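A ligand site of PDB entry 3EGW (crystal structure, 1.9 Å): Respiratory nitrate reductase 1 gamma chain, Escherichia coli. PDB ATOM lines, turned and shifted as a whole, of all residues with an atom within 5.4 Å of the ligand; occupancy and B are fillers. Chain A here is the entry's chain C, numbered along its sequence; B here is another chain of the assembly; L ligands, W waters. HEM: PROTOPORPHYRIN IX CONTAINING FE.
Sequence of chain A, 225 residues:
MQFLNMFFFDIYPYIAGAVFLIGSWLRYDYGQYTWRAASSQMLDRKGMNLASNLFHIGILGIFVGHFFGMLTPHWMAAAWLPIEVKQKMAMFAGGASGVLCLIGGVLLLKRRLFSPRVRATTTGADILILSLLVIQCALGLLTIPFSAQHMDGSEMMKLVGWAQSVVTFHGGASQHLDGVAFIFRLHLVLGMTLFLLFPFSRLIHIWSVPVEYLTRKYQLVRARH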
ATOM      1  N   ALA A  37      27.915  18.028   5.936  1.00  0.00           N
ATOM      2  CA  ALA A  37      27.944  18.834   4.715  1.00  0.00           C
ATOM      3  C   ALA A  37      29.098  18.428   3.807  1.00  0.00           C
ATOM      4  O   ALA A  37      29.083  18.683   2.609  1.00  0.00           O
ATOM      5  CB  ALA A  37      28.063  20.310   5.075  1.00  0.00           C
ATOM      6  N   ALA A  38      30.109  17.783   4.394  1.00  0.00           N
ATOM      7  CA  ALA A  38      31.276  17.322   3.661  1.00  0.00           C
ATOM      8  C   ALA A  38      32.044  18.455   2.986  1.00  0.00           C
ATOM      9  O   ALA A  38      32.383  18.382   1.799  1.00  0.00           O
ATOM     10  CB  ALA A  38      30.873  16.282   2.627  1.00  0.00           C
ATOM     11  N   SER A  39      32.337  19.489   3.759  1.00  0.00           N
ATOM     12  CA  SER A  39      33.072  20.635   3.250  1.00  0.00           C
ATOM     13  C   SER A  39      34.422  20.190   2.694  1.00  0.00           C
ATOM     14  O   SER A  39      35.061  19.296   3.240  1.00  0.00           O
ATOM     15  CB  SER A  39      33.312  21.653   4.361  1.00  0.00           C
ATOM     16  OG  SER A  39      34.183  22.683   3.915  1.00  0.00           O
ATOM     17  N   SER A  40      34.850  20.821   1.606  1.00  0.00           N
ATOM     18  CA  SER A  40      36.142  20.519   0.995  1.00  0.00           C
ATOM     19  C   SER A  40      36.938  21.811   0.897  1.00  0.00           C
ATOM     20  O   SER A  40      38.025  21.840   0.320  1.00  0.00           O
ATOM     21  CB  SER A  40      35.916  19.930  -0.409  1.00  0.00           C
ATOM     22  OG  SER A  40      35.243  20.854  -1.250  1.00  0.00           O
ATOM     23  N   GLN A  41      36.391  22.875   1.477  1.00  0.00           N
ATOM     24  CA  GLN A  41      37.003  24.199   1.431  1.00  0.00           C
ATOM     25  C   GLN A  41      38.452  24.290   1.919  1.00  0.00           C
ATOM     26  O   GLN A  41      39.291  24.912   1.265  1.00  0.00           O
ATOM     27  CB  GLN A  41      36.144  25.193   2.218  1.00  0.00           C
ATOM     28  CG  GLN A  41      36.508  26.656   1.948  1.00  0.00           C
ATOM     29  CD  GLN A  41      35.741  27.633   2.827  1.00  0.00           C
ATOM     30  OE1 GLN A  41      34.883  27.246   3.616  1.00  0.00           O
ATOM     31  NE2 GLN A  41      36.071  28.917   2.695  1.00  0.00           N
ATOM     32  N   MET A  48      36.094  29.194  -3.927  1.00  0.00           N
ATOM     33  CA  MET A  48      34.956  28.705  -3.175  1.00  0.00           C
ATOM     34  C   MET A  48      33.983  29.764  -2.674  1.00  0.00           C
ATOM     35  O   MET A  48      32.771  29.553  -2.674  1.00  0.00           O
ATOM     36  CB  MET A  48      35.416  27.864  -1.974  1.00  0.00           C
ATOM     37  CG  MET A  48      35.627  26.409  -2.310  1.00  0.00           C
ATOM     38  SD  MET A  48      34.142  25.709  -3.062  1.00  0.00           S
ATOM     39  CE  MET A  48      33.408  24.885  -1.692  1.00  0.00           C
ATOM     40  N   SER A  52      30.496  28.822  -4.157  1.00  0.00           N
ATOM     41  CA  SER A  52      29.514  28.302  -3.205  1.00  0.00           C
ATOM     42  C   SER A  52      28.396  29.288  -2.893  1.00  0.00           C
ATOM     43  O   SER A  52      27.234  28.894  -2.775  1.00  0.00           O
ATOM     44  CB  SER A  52      30.197  27.867  -1.911  1.00  0.00           C
ATOM     45  OG  SER A  52      29.275  27.145  -1.104  1.00  0.00           O
ATOM     46  N   PHE A  55      26.088  29.531  -5.984  1.00  0.00           N
ATOM     47  CA  PHE A  55      25.306  28.321  -6.055  1.00  0.00           C
ATOM     48  C   PHE A  55      24.229  28.222  -4.977  1.00  0.00           C
ATOM     49  O   PHE A  55      23.064  27.977  -5.287  1.00  0.00           O
ATOM     50  CB  PHE A  55      26.211  27.082  -5.988  1.00  0.00           C
ATOM     51  CG  PHE A  55      25.459  25.792  -5.879  1.00  0.00           C
ATOM     52  CD1 PHE A  55      25.194  25.232  -4.639  1.00  0.00           C
ATOM     53  CD2 PHE A  55      24.975  25.164  -7.023  1.00  0.00           C
ATOM     54  CE1 PHE A  55      24.443  24.073  -4.534  1.00  0.00           C
ATOM     55  CE2 PHE A  55      24.217  24.007  -6.924  1.00  0.00           C
ATOM     56  CZ  PHE A  55      23.961  23.455  -5.677  1.00  0.00           C
ATOM     57  N   HIS A  56      24.603  28.411  -3.710  1.00  0.00           N
ATOM     58  CA  HIS A  56      23.616  28.296  -2.647  1.00  0.00           C
ATOM     59  C   HIS A  56      22.566  29.407  -2.635  1.00  0.00           C
ATOM     60  O   HIS A  56      21.389  29.126  -2.427  1.00  0.00           O
ATOM     61  CB  HIS A  56      24.295  28.206  -1.271  1.00  0.00           C
ATOM     62  CG  HIS A  56      24.807  26.830  -0.963  1.00  0.00           C
ATOM     63  ND1 HIS A  56      26.111  26.449  -1.186  1.00  0.00           N
ATOM     64  CD2 HIS A  56      24.171  25.727  -0.482  1.00  0.00           C
ATOM     65  CE1 HIS A  56      26.260  25.179  -0.867  1.00  0.00           C
ATOM     66  NE2 HIS A  56      25.099  24.719  -0.438  1.00  0.00           N
ATOM     67  N   ILE A  59      20.296  28.483  -5.579  1.00  0.00           N
ATOM     68  CA  ILE A  59      19.473  27.295  -5.334  1.00  0.00           C
ATOM     69  C   ILE A  59      18.405  27.541  -4.267  1.00  0.00           C
ATOM     70  O   ILE A  59      17.309  26.954  -4.330  1.00  0.00           O
ATOM     71  CB  ILE A  59      20.340  26.078  -4.908  1.00  0.00           C
ATOM     72  CG1 ILE A  59      19.547  24.780  -5.094  1.00  0.00           C
ATOM     73  CG2 ILE A  59      20.736  26.179  -3.454  1.00  0.00           C
ATOM     74  CD1 ILE A  59      19.453  24.330  -6.512  1.00  0.00           C
ATOM     75  N   LEU A  60      18.703  28.377  -3.280  1.00  0.00           N
ATOM     76  CA  LEU A  60      17.734  28.666  -2.242  1.00  0.00           C
ATOM     77  C   LEU A  60      16.624  29.553  -2.814  1.00  0.00           C
ATOM     78  O   LEU A  60      15.468  29.427  -2.425  1.00  0.00           O
ATOM     79  CB  LEU A  60      18.416  29.319  -1.029  1.00  0.00           C
ATOM     80  CG  LEU A  60      19.272  28.312  -0.248  1.00  0.00           C
ATOM     81  CD1 LEU A  60      20.038  29.002   0.874  1.00  0.00           C
ATOM     82  CD2 LEU A  60      18.357  27.227   0.313  1.00  0.00           C
ATOM     83  N   LEU A 108      31.717  25.074  -9.207  1.00  0.00           N
ATOM     84  CA  LEU A 108      31.953  24.042  -8.206  1.00  0.00           C
ATOM     85  C   LEU A 108      32.294  22.701  -8.855  1.00  0.00           C
ATOM     86  O   LEU A 108      33.160  21.981  -8.379  1.00  0.00           O
ATOM     87  CB  LEU A 108      30.723  23.861  -7.309  1.00  0.00           C
ATOM     88  CG  LEU A 108      30.397  25.012  -6.347  1.00  0.00           C
ATOM     89  CD1 LEU A 108      29.010  24.793  -5.772  1.00  0.00           C
ATOM     90  CD2 LEU A 108      31.453  25.062  -5.239  1.00  0.00           C
ATOM     91  N   ARG A 111      35.758  22.745 -10.229  1.00  0.00           N
ATOM     92  CA  ARG A 111      36.666  22.597  -9.086  1.00  0.00           C
ATOM     93  C   ARG A 111      36.760  21.141  -8.618  1.00  0.00           C
ATOM     94  O   ARG A 111      37.856  20.619  -8.460  1.00  0.00           O
ATOM     95  CB  ARG A 111      36.193  23.477  -7.936  1.00  0.00           C
ATOM     96  CG  ARG A 111      36.971  23.319  -6.627  1.00  0.00           C
ATOM     97  CD  ARG A 111      36.515  24.371  -5.629  1.00  0.00           C
ATOM     98  NE  ARG A 111      37.126  24.242  -4.306  1.00  0.00           N
ATOM     99  CZ  ARG A 111      36.790  23.324  -3.404  1.00  0.00           C
ATOM    100  NH1 ARG A 111      37.413  23.297  -2.228  1.00  0.00           N
ATOM    101  NH2 ARG A 111      35.825  22.443  -3.671  1.00  0.00           N
ATOM    102  N   ARG A 112      35.613  20.509  -8.416  1.00  0.00           N
ATOM    103  CA  ARG A 112      35.583  19.126  -7.943  1.00  0.00           C
ATOM    104  C   ARG A 112      36.283  18.173  -8.908  1.00  0.00           C
ATOM    105  O   ARG A 112      36.953  17.235  -8.486  1.00  0.00           O
ATOM    106  CB  ARG A 112      34.131  18.670  -7.718  1.00  0.00           C
ATOM    107  CG  ARG A 112      33.971  17.248  -7.164  1.00  0.00           C
ATOM    108  CD  ARG A 112      32.627  17.080  -6.456  1.00  0.00           C
ATOM    109  NE  ARG A 112      32.554  17.980  -5.303  1.00  0.00           N
ATOM    110  CZ  ARG A 112      33.226  17.803  -4.170  1.00  0.00           C
ATOM    111  NH1 ARG A 112      34.011  16.747  -4.017  1.00  0.00           N
ATOM    112  NH2 ARG A 112      33.137  18.698  -3.200  1.00  0.00           N
ATOM    113  N   ASP A 126      29.412  12.548  -4.802  1.00  0.00           N
ATOM    114  CA  ASP A 126      29.530  14.000  -4.818  1.00  0.00           C
ATOM    115  C   ASP A 126      29.548  14.526  -6.259  1.00  0.00           C
ATOM    116  O   ASP A 126      28.947  15.552  -6.556  1.00  0.00           O
ATOM    117  CB  ASP A 126      30.806  14.474  -4.106  1.00  0.00           C
ATOM    118  CG  ASP A 126      30.846  14.029  -2.653  1.00  0.00           C
ATOM    119  OD1 ASP A 126      29.818  14.150  -1.956  1.00  0.00           O
ATOM    120  OD2 ASP A 126      31.920  13.567  -2.208  1.00  0.00           O
ATOM    121  N   ILE A 129      25.830  13.769  -7.867  1.00  0.00           N
ATOM    122  CA  ILE A 129      24.782  14.660  -7.393  1.00  0.00           C
ATOM    123  C   ILE A 129      24.944  16.101  -7.882  1.00  0.00           C
ATOM    124  O   ILE A 129      23.954  16.749  -8.230  1.00  0.00           O
ATOM    125  CB  ILE A 129      24.680  14.624  -5.839  1.00  0.00           C
ATOM    126  CG1 ILE A 129      23.267  15.021  -5.407  1.00  0.00           C
ATOM    127  CG2 ILE A 129      25.692  15.562  -5.212  1.00  0.00           C
ATOM    128  CD1 ILE A 129      22.197  13.998  -5.768  1.00  0.00           C
ATOM    129  N   LEU A 130      26.174  16.604  -7.932  1.00  0.00           N
ATOM    130  CA  LEU A 130      26.397  17.973  -8.400  1.00  0.00           C
ATOM    131  C   LEU A 130      26.162  18.078  -9.904  1.00  0.00           C
ATOM    132  O   LEU A 130      25.642  19.082 -10.392  1.00  0.00           O
ATOM    133  CB  LEU A 130      27.818  18.426  -8.062  1.00  0.00           C
ATOM    134  CG  LEU A 130      28.196  19.829  -8.549  1.00  0.00           C
ATOM    135  CD1 LEU A 130      27.266  20.869  -7.931  1.00  0.00           C
ATOM    136  CD2 LEU A 130      29.655  20.112  -8.169  1.00  0.00           C
ATOM    137  N   LEU A 133      22.535  18.234 -10.498  1.00  0.00           N
ATOM    138  CA  LEU A 133      21.977  19.526 -10.088  1.00  0.00           C
ATOM    139  C   LEU A 133      22.279  20.575 -11.154  1.00  0.00           C
ATOM    140  O   LEU A 133      21.436  21.420 -11.458  1.00  0.00           O
ATOM    141  CB  LEU A 133      22.555  19.972  -8.738  1.00  0.00           C
ATOM    142  CG  LEU A 133      22.010  19.258  -7.501  1.00  0.00           C
ATOM    143  CD1 LEU A 133      22.911  19.527  -6.303  1.00  0.00           C
ATOM    144  CD2 LEU A 133      20.589  19.730  -7.229  1.00  0.00           C
ATOM    145  N   ARG A 202      25.142  13.666  -0.212  1.00  0.00           N
ATOM    146  CA  ARG A 202      25.448  14.735   0.724  1.00  0.00           C
ATOM    147  C   ARG A 202      24.263  15.685   0.919  1.00  0.00           C
ATOM    148  O   ARG A 202      24.263  16.494   1.845  1.00  0.00           O
ATOM    149  CB  ARG A 202      26.649  15.535   0.231  1.00  0.00           C
ATOM    150  CG  ARG A 202      26.382  16.292  -1.074  1.00  0.00           C
ATOM    151  CD  ARG A 202      27.670  16.783  -1.675  1.00  0.00           C
ATOM    152  NE  ARG A 202      28.412  17.633  -0.752  1.00  0.00           N
ATOM    153  CZ  ARG A 202      29.679  17.999  -0.923  1.00  0.00           C
ATOM    154  NH1 ARG A 202      30.342  17.582  -1.990  1.00  0.00           N
ATOM    155  NH2 ARG A 202      30.269  18.775  -0.026  1.00  0.00           N
ATOM    156  N   LEU A 203      23.257  15.592   0.055  1.00  0.00           N
ATOM    157  CA  LEU A 203      22.106  16.486   0.168  1.00  0.00           C
ATOM    158  C   LEU A 203      21.407  16.397   1.521  1.00  0.00           C
ATOM    159  O   LEU A 203      20.603  17.266   1.860  1.00  0.00           O
ATOM    160  CB  LEU A 203      21.096  16.215  -0.951  1.00  0.00           C
ATOM    161  CG  LEU A 203      21.644  16.423  -2.366  1.00  0.00           C
ATOM    162  CD1 LEU A 203      20.510  16.284  -3.371  1.00  0.00           C
ATOM    163  CD2 LEU A 203      22.281  17.805  -2.491  1.00  0.00           C
ATOM    164  N   HIS A 205      22.436  17.242   4.109  1.00  0.00           N
ATOM    165  CA  HIS A 205      22.815  18.433   4.894  1.00  0.00           C
ATOM    166  C   HIS A 205      21.693  19.465   4.895  1.00  0.00           C
ATOM    167  O   HIS A 205      21.575  20.254   5.829  1.00  0.00           O
ATOM    168  CB  HIS A 205      24.141  19.078   4.407  1.00  0.00           C
ATOM    169  CG  HIS A 205      24.065  19.822   3.094  1.00  0.00           C
ATOM    170  ND1 HIS A 205      23.807  19.195   1.890  1.00  0.00           N
ATOM    171  CD2 HIS A 205      24.339  21.119   2.783  1.00  0.00           C
ATOM    172  CE1 HIS A 205      23.939  20.060   0.904  1.00  0.00           C
ATOM    173  NE2 HIS A 205      24.256  21.235   1.416  1.00  0.00           N
ATOM    174  N   ILE A 206      20.857  19.436   3.862  1.00  0.00           N
ATOM    175  CA  ILE A 206      19.751  20.376   3.745  1.00  0.00           C
ATOM    176  C   ILE A 206      18.787  20.256   4.921  1.00  0.00           C
ATOM    177  O   ILE A 206      18.296  21.270   5.423  1.00  0.00           O
ATOM    178  CB  ILE A 206      18.987  20.166   2.417  1.00  0.00           C
ATOM    179  CG1 ILE A 206      19.957  20.285   1.235  1.00  0.00           C
ATOM    180  CG2 ILE A 206      17.881  21.198   2.275  1.00  0.00           C
ATOM    181  CD1 ILE A 206      19.387  19.787  -0.089  1.00  0.00           C
ATOM    182  N   VAL A 209      19.537  22.584   8.086  1.00  0.00           N
ATOM    183  CA  VAL A 209      19.664  24.045   8.076  1.00  0.00           C
ATOM    184  C   VAL A 209      19.538  24.493   9.533  1.00  0.00           C
ATOM    185  O   VAL A 209      18.506  24.291  10.179  1.00  0.00           O
ATOM    186  CB  VAL A 209      18.578  24.699   7.176  1.00  0.00           C
ATOM    187  CG1 VAL A 209      17.211  24.134   7.526  1.00  0.00           C
ATOM    188  CG2 VAL A 209      18.601  26.216   7.346  1.00  0.00           C
ATOM    189  N   PRO A 210      20.601  25.098  10.089  1.00  0.00           N
ATOM    190  CA  PRO A 210      20.698  25.578  11.479  1.00  0.00           C
ATOM    191  C   PRO A 210      19.785  26.709  11.942  1.00  0.00           C
ATOM    192  O   PRO A 210      20.268  27.722  12.457  1.00  0.00           O
ATOM    193  CB  PRO A 210      22.173  25.954  11.597  1.00  0.00           C
ATOM    194  CG  PRO A 210      22.471  26.510  10.241  1.00  0.00           C
ATOM    195  CD  PRO A 210      21.801  25.495   9.322  1.00  0.00           C
ATOM    196  N   ILE B  88      28.045  30.841   6.195  1.00  0.00           N
ATOM    197  CA  ILE B  88      28.044  29.389   6.152  1.00  0.00           C
ATOM    198  C   ILE B  88      28.321  28.669   4.831  1.00  0.00           C
ATOM    199  O   ILE B  88      28.807  27.536   4.836  1.00  0.00           O
ATOM    200  CB  ILE B  88      26.739  28.840   6.761  1.00  0.00           C
ATOM    201  CG1 ILE B  88      26.960  27.422   7.290  1.00  0.00           C
ATOM    202  CG2 ILE B  88      25.616  28.873   5.717  1.00  0.00           C
ATOM    203  CD1 ILE B  88      25.935  26.989   8.326  1.00  0.00           C
ATOM    204  N   PHE B  89      28.017  29.298   3.696  1.00  0.00           N
ATOM    205  CA  PHE B  89      28.249  28.626   2.422  1.00  0.00           C
ATOM    206  C   PHE B  89      29.724  28.542   2.066  1.00  0.00           C
ATOM    207  O   PHE B  89      30.145  27.666   1.303  1.00  0.00           O
ATOM    208  CB  PHE B  89      27.463  29.331   1.308  1.00  0.00           C
ATOM    209  CG  PHE B  89      25.987  29.376   1.564  1.00  0.00           C
ATOM    210  CD1 PHE B  89      25.299  28.233   1.941  1.00  0.00           C
ATOM    211  CD2 PHE B  89      25.281  30.570   1.458  1.00  0.00           C
ATOM    212  CE1 PHE B  89      23.931  28.270   2.210  1.00  0.00           C
ATOM    213  CE2 PHE B  89      23.915  30.626   1.713  1.00  0.00           C
ATOM    214  CZ  PHE B  89      23.232  29.472   2.096  1.00  0.00           C
ATOM    215  N   ALA B  90      30.516  29.438   2.645  1.00  0.00           N
ATOM    216  CA  ALA B  90      31.961  29.479   2.429  1.00  0.00           C
ATOM    217  C   ALA B  90      32.576  30.349   3.519  1.00  0.00           C
ATOM    218  O   ALA B  90      32.574  31.570   3.420  1.00  0.00           O
ATOM    219  CB  ALA B  90      32.281  30.052   1.050  1.00  0.00           C
ATOM    220  N   GLY B 219      29.333  19.398  10.282  1.00  0.00           N
ATOM    221  CA  GLY B 219      30.414  19.858   9.420  1.00  0.00           C
ATOM    222  C   GLY B 219      30.284  21.271   8.876  1.00  0.00           C
ATOM    223  O   GLY B 219      30.726  21.544   7.755  1.00  0.00           O
ATOM    224  N   TRP B 220      29.680  22.169   9.640  1.00  0.00           N
ATOM    225  CA  TRP B 220      29.507  23.557   9.219  1.00  0.00           C
ATOM    226  C   TRP B 220      30.837  24.306   9.232  1.00  0.00           C
ATOM    227  O   TRP B 220      30.959  25.400   8.665  1.00  0.00           O
ATOM    228  CB  TRP B 220      28.507  24.260  10.137  1.00  0.00           C
ATOM    229  CG  TRP B 220      27.102  23.698  10.115  1.00  0.00           C
ATOM    230  CD1 TRP B 220      26.286  23.491  11.190  1.00  0.00           C
ATOM    231  CD2 TRP B 220      26.339  23.292   8.958  1.00  0.00           C
ATOM    232  NE1 TRP B 220      25.067  22.993  10.778  1.00  0.00           N
ATOM    233  CE2 TRP B 220      25.077  22.859   9.417  1.00  0.00           C
ATOM    234  CE3 TRP B 220      26.602  23.256   7.573  1.00  0.00           C
ATOM    235  CZ2 TRP B 220      24.069  22.391   8.549  1.00  0.00           C
ATOM    236  CZ3 TRP B 220      25.601  22.786   6.711  1.00  0.00           C
ATOM    237  CH2 TRP B 220      24.352  22.371   7.205  1.00  0.00           C
ATOM    238  N   ARG B 221      31.844  23.701   9.863  1.00  0.00           N
ATOM    239  CA  ARG B 221      33.198  24.261   9.961  1.00  0.00           C
ATOM    240  C   ARG B 221      33.345  25.754  10.277  1.00  0.00           C
ATOM    241  O   ARG B 221      34.211  26.441   9.730  1.00  0.00           O
ATOM    242  CB  ARG B 221      34.011  23.892   8.699  1.00  0.00           C
ATOM    243  CG  ARG B 221      33.330  24.165   7.350  1.00  0.00           C
ATOM    244  CD  ARG B 221      33.646  25.559   6.826  1.00  0.00           C
ATOM    245  NE  ARG B 221      33.099  25.778   5.478  1.00  0.00           N
ATOM    246  CZ  ARG B 221      31.858  26.185   5.215  1.00  0.00           C
ATOM    247  NH1 ARG B 221      31.007  26.434   6.200  1.00  0.00           N
ATOM    248  NH2 ARG B 221      31.485  26.362   3.952  1.00  0.00           N
HETATM  249  CHA HEM L   1      27.835  22.011  -0.023  1.00  0.00           C
HETATM  250  CHB HEM L   1      25.575  24.423   3.489  1.00  0.00           C
HETATM  251  CHC HEM L   1      21.445  23.976   0.988  1.00  0.00           C
HETATM  252  CHD HEM L   1      23.689  21.536  -2.496  1.00  0.00           C
HETATM  253  C1A HEM L   1      27.604  22.695   1.158  1.00  0.00           C
HETATM  254  C2A HEM L   1      28.578  23.045   2.196  1.00  0.00           C
HETATM  255  C3A HEM L   1      27.943  23.712   3.162  1.00  0.00           C
HETATM  256  C4A HEM L   1      26.548  23.804   2.760  1.00  0.00           C
HETATM  257  CMA HEM L   1      28.497  24.315   4.497  1.00  0.00           C
HETATM  258  CAA HEM L   1      30.084  22.666   2.141  1.00  0.00           C
HETATM  259  CBA HEM L   1      30.896  23.753   1.312  1.00  0.00           C
HETATM  260  CGA HEM L   1      32.425  23.652   1.447  1.00  0.00           C
HETATM  261  O1A HEM L   1      32.965  24.355   2.339  1.00  0.00           O
HETATM  262  O2A HEM L   1      33.015  22.848   0.658  1.00  0.00           O
HETATM  263  C1B HEM L   1      24.240  24.514   3.125  1.00  0.00           C
HETATM  264  C2B HEM L   1      23.192  25.176   3.904  1.00  0.00           C
HETATM  265  C3B HEM L   1      22.029  25.048   3.214  1.00  0.00           C
HETATM  266  C4B HEM L   1      22.349  24.319   1.982  1.00  0.00           C
HETATM  267  CMB HEM L   1      23.469  25.858   5.286  1.00  0.00           C
HETATM  268  CAB HEM L   1      20.583  25.574   3.589  1.00  0.00           C
HETATM  269  CBB HEM L   1      20.271  26.863   3.929  1.00  0.00           C
HETATM  270  C1C HEM L   1      21.669  23.283  -0.172  1.00  0.00           C
HETATM  271  C2C HEM L   1      20.665  22.948  -1.186  1.00  0.00           C
HETATM  272  C3C HEM L   1      21.293  22.252  -2.166  1.00  0.00           C
HETATM  273  C4C HEM L   1      22.702  22.158  -1.766  1.00  0.00           C
HETATM  274  CMC HEM L   1      19.147  23.359  -1.079  1.00  0.00           C
HETATM  275  CAC HEM L   1      20.770  21.623  -3.512  1.00  0.00           C
HETATM  276  CBC HEM L   1      19.596  20.938  -3.522  1.00  0.00           C
HETATM  277  C1D HEM L   1      25.016  21.447  -2.138  1.00  0.00           C
HETATM  278  C2D HEM L   1      26.055  20.787  -2.938  1.00  0.00           C
HETATM  279  C3D HEM L   1      27.206  20.927  -2.247  1.00  0.00           C
HETATM  280  C4D HEM L   1      26.905  21.673  -1.001  1.00  0.00           C
HETATM  281  CMD HEM L   1      25.824  20.066  -4.303  1.00  0.00           C
HETATM  282  CAD HEM L   1      28.668  20.469  -2.578  1.00  0.00           C
HETATM  283  CBD HEM L   1      29.425  21.386  -3.613  1.00  0.00           C
HETATM  284  CGD HEM L   1      30.715  20.758  -4.156  1.00  0.00           C
HETATM  285  O1D HEM L   1      31.806  21.238  -3.691  1.00  0.00           O
HETATM  286  O2D HEM L   1      30.556  19.835  -5.029  1.00  0.00           O
HETATM  287  NA  HEM L   1      26.366  23.174   1.529  1.00  0.00           N
HETATM  288  NB  HEM L   1      23.701  23.997   1.947  1.00  0.00           N
HETATM  289  NC  HEM L   1      22.906  22.794  -0.543  1.00  0.00           N
HETATM  290  ND  HEM L   1      25.579  21.980  -0.969  1.00  0.00           N
HETATM  291 FE   HEM L   1      24.674  22.993   0.497  1.00  0.00          FE
HETATM  292  O   HOH W   1      29.040  17.580  -4.709  1.00  0.00           O
HETATM  293  O   HOH W   2      32.479  20.887  -1.109  1.00  0.00           O
HETATM  294  O   HOH W   3      26.840  19.225   1.154  1.00  0.00           O
HETATM  295  O   HOH W   4      33.733  21.870  -5.689  1.00  0.00           O
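An oxygen (O2A) of the ligand is in hydrogen-bond range of the backbone NH of Gln 41 (3.5 Å).
NE2 of His 56 binds FE of the ligand (2.0 Å).
NE2 of His 205 binds FE of the ligand, at 2.0 Å.
An oxygen (O2A) of the ligand sits at hydrogen-bond distance from the backbone NH (N) of Ser 40.
O1A of the ligand lies within hydrogen-bond range of OG of Ser 39, 2.6 Å away.
An oxygen (O2D) of the ligand is in salt-bridge range of the guanidinium group (NH1) of Arg 202 (3.8 Å).
NH2 of Arg 221 of chain B is in salt-bridge range of O1A of the ligand, at 3.0 Å.
An oxygen (O2D) of the ligand lies within salt-bridge range of the guanidinium group of Arg 112 (2.7 Å).
OG of Ser 52 sits at hydrogen-bond distance from O of Phe 89 of chain B, at 2.6 Å.
O of Arg 202 sits at hydrogen-bond distance from ND1 of His 205 (2.7 Å).
O of Ala 37 is in hydrogen-bond range of NH2 of Arg 202.
The backbone carbonyl oxygen (O) of Phe 89 of chain B sits at hydrogen-bond distance from the guanidinium group (NH2) of Arg 221 of chain B, 3.2 Å away.
NH1 of Arg 202 lies within salt-bridge range of OD1 of Asp 126 (3.5 Å).
A ring nitrogen (ND1) of His 56 is in hydrogen-bond range of the backbone carbonyl oxygen of Ser 52, 3.1 Å away.
The side-chain hydroxyl (OG) of Ser 39 is in hydrogen-bond range of the backbone NH (N) of Gln 41 (3.3 Å).
The side-chain sulfur of Met 48 lies close to the guanidinium group of Arg 111 (3.6 Å).
Residues that only touch the ligand: Met 48 (3.1 Å), Ile 88 of chain B (3.3 Å), Leu 130 (3.3 Å), Phe 55 (3.3 Å), Leu 133 (3.6 Å), Ile 206 (3.6 Å), Phe 89 of chain B (3.6 Å), Trp 220 of chain B (3.6 Å), Leu 60 (3.7 Å), Ile 59 (3.7 Å), Val 209 (3.9 Å), Ala 37 (3.9 Å) and Leu 203 (3.99 Å).
21 residues have an atom within 4 Å of the ligand: Ala 37, Ser 39, Ser 40, Gln 41, Met 48, Phe 55, His 56, Ile 59, Leu 60, Arg 112, Leu 130, Leu 133, Arg 202, Leu 203, His 205, Ile 206, Val 209, Ile 88 of chain B, Phe 89 of chain B, Trp 220 of chain B and Arg 221 of chain B.
Along chain A the residues within 4 Å of the ligand span positions 37 to 209.
Water W2 lies within hydrogen-bond range of an oxygen (O1D) of the ligand (2.7 Å), the side-chain hydroxyl (OG) of Ser 40 (2.8 Å), the guanidinium group (NH2) of Arg 112 (3.1 Å) and the guanidinium group (NH2) of Arg 202 (3.2 Å).
Water W1 lies within hydrogen-bond range of an oxygen (O2D) of the ligand (2.7 Å), the backbone carbonyl oxygen of Asp 126 (2.7 Å) and the guanidinium group of Arg 202 (3.0 Å).
Water W4 lies within hydrogen-bond range of O of Leu 108 (2.8 Å), O1D of the ligand (2.8 Å) and NH2 of Arg 111 (3.0 Å).
Water W3 lies within hydrogen-bond range of the backbone carbonyl oxygen (O) of Ala 37 (2.7 Å), the guanidinium group (NE) of Arg 202 (2.9 Å) and a ring nitrogen (ND1) of His 205 (3.1 Å).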
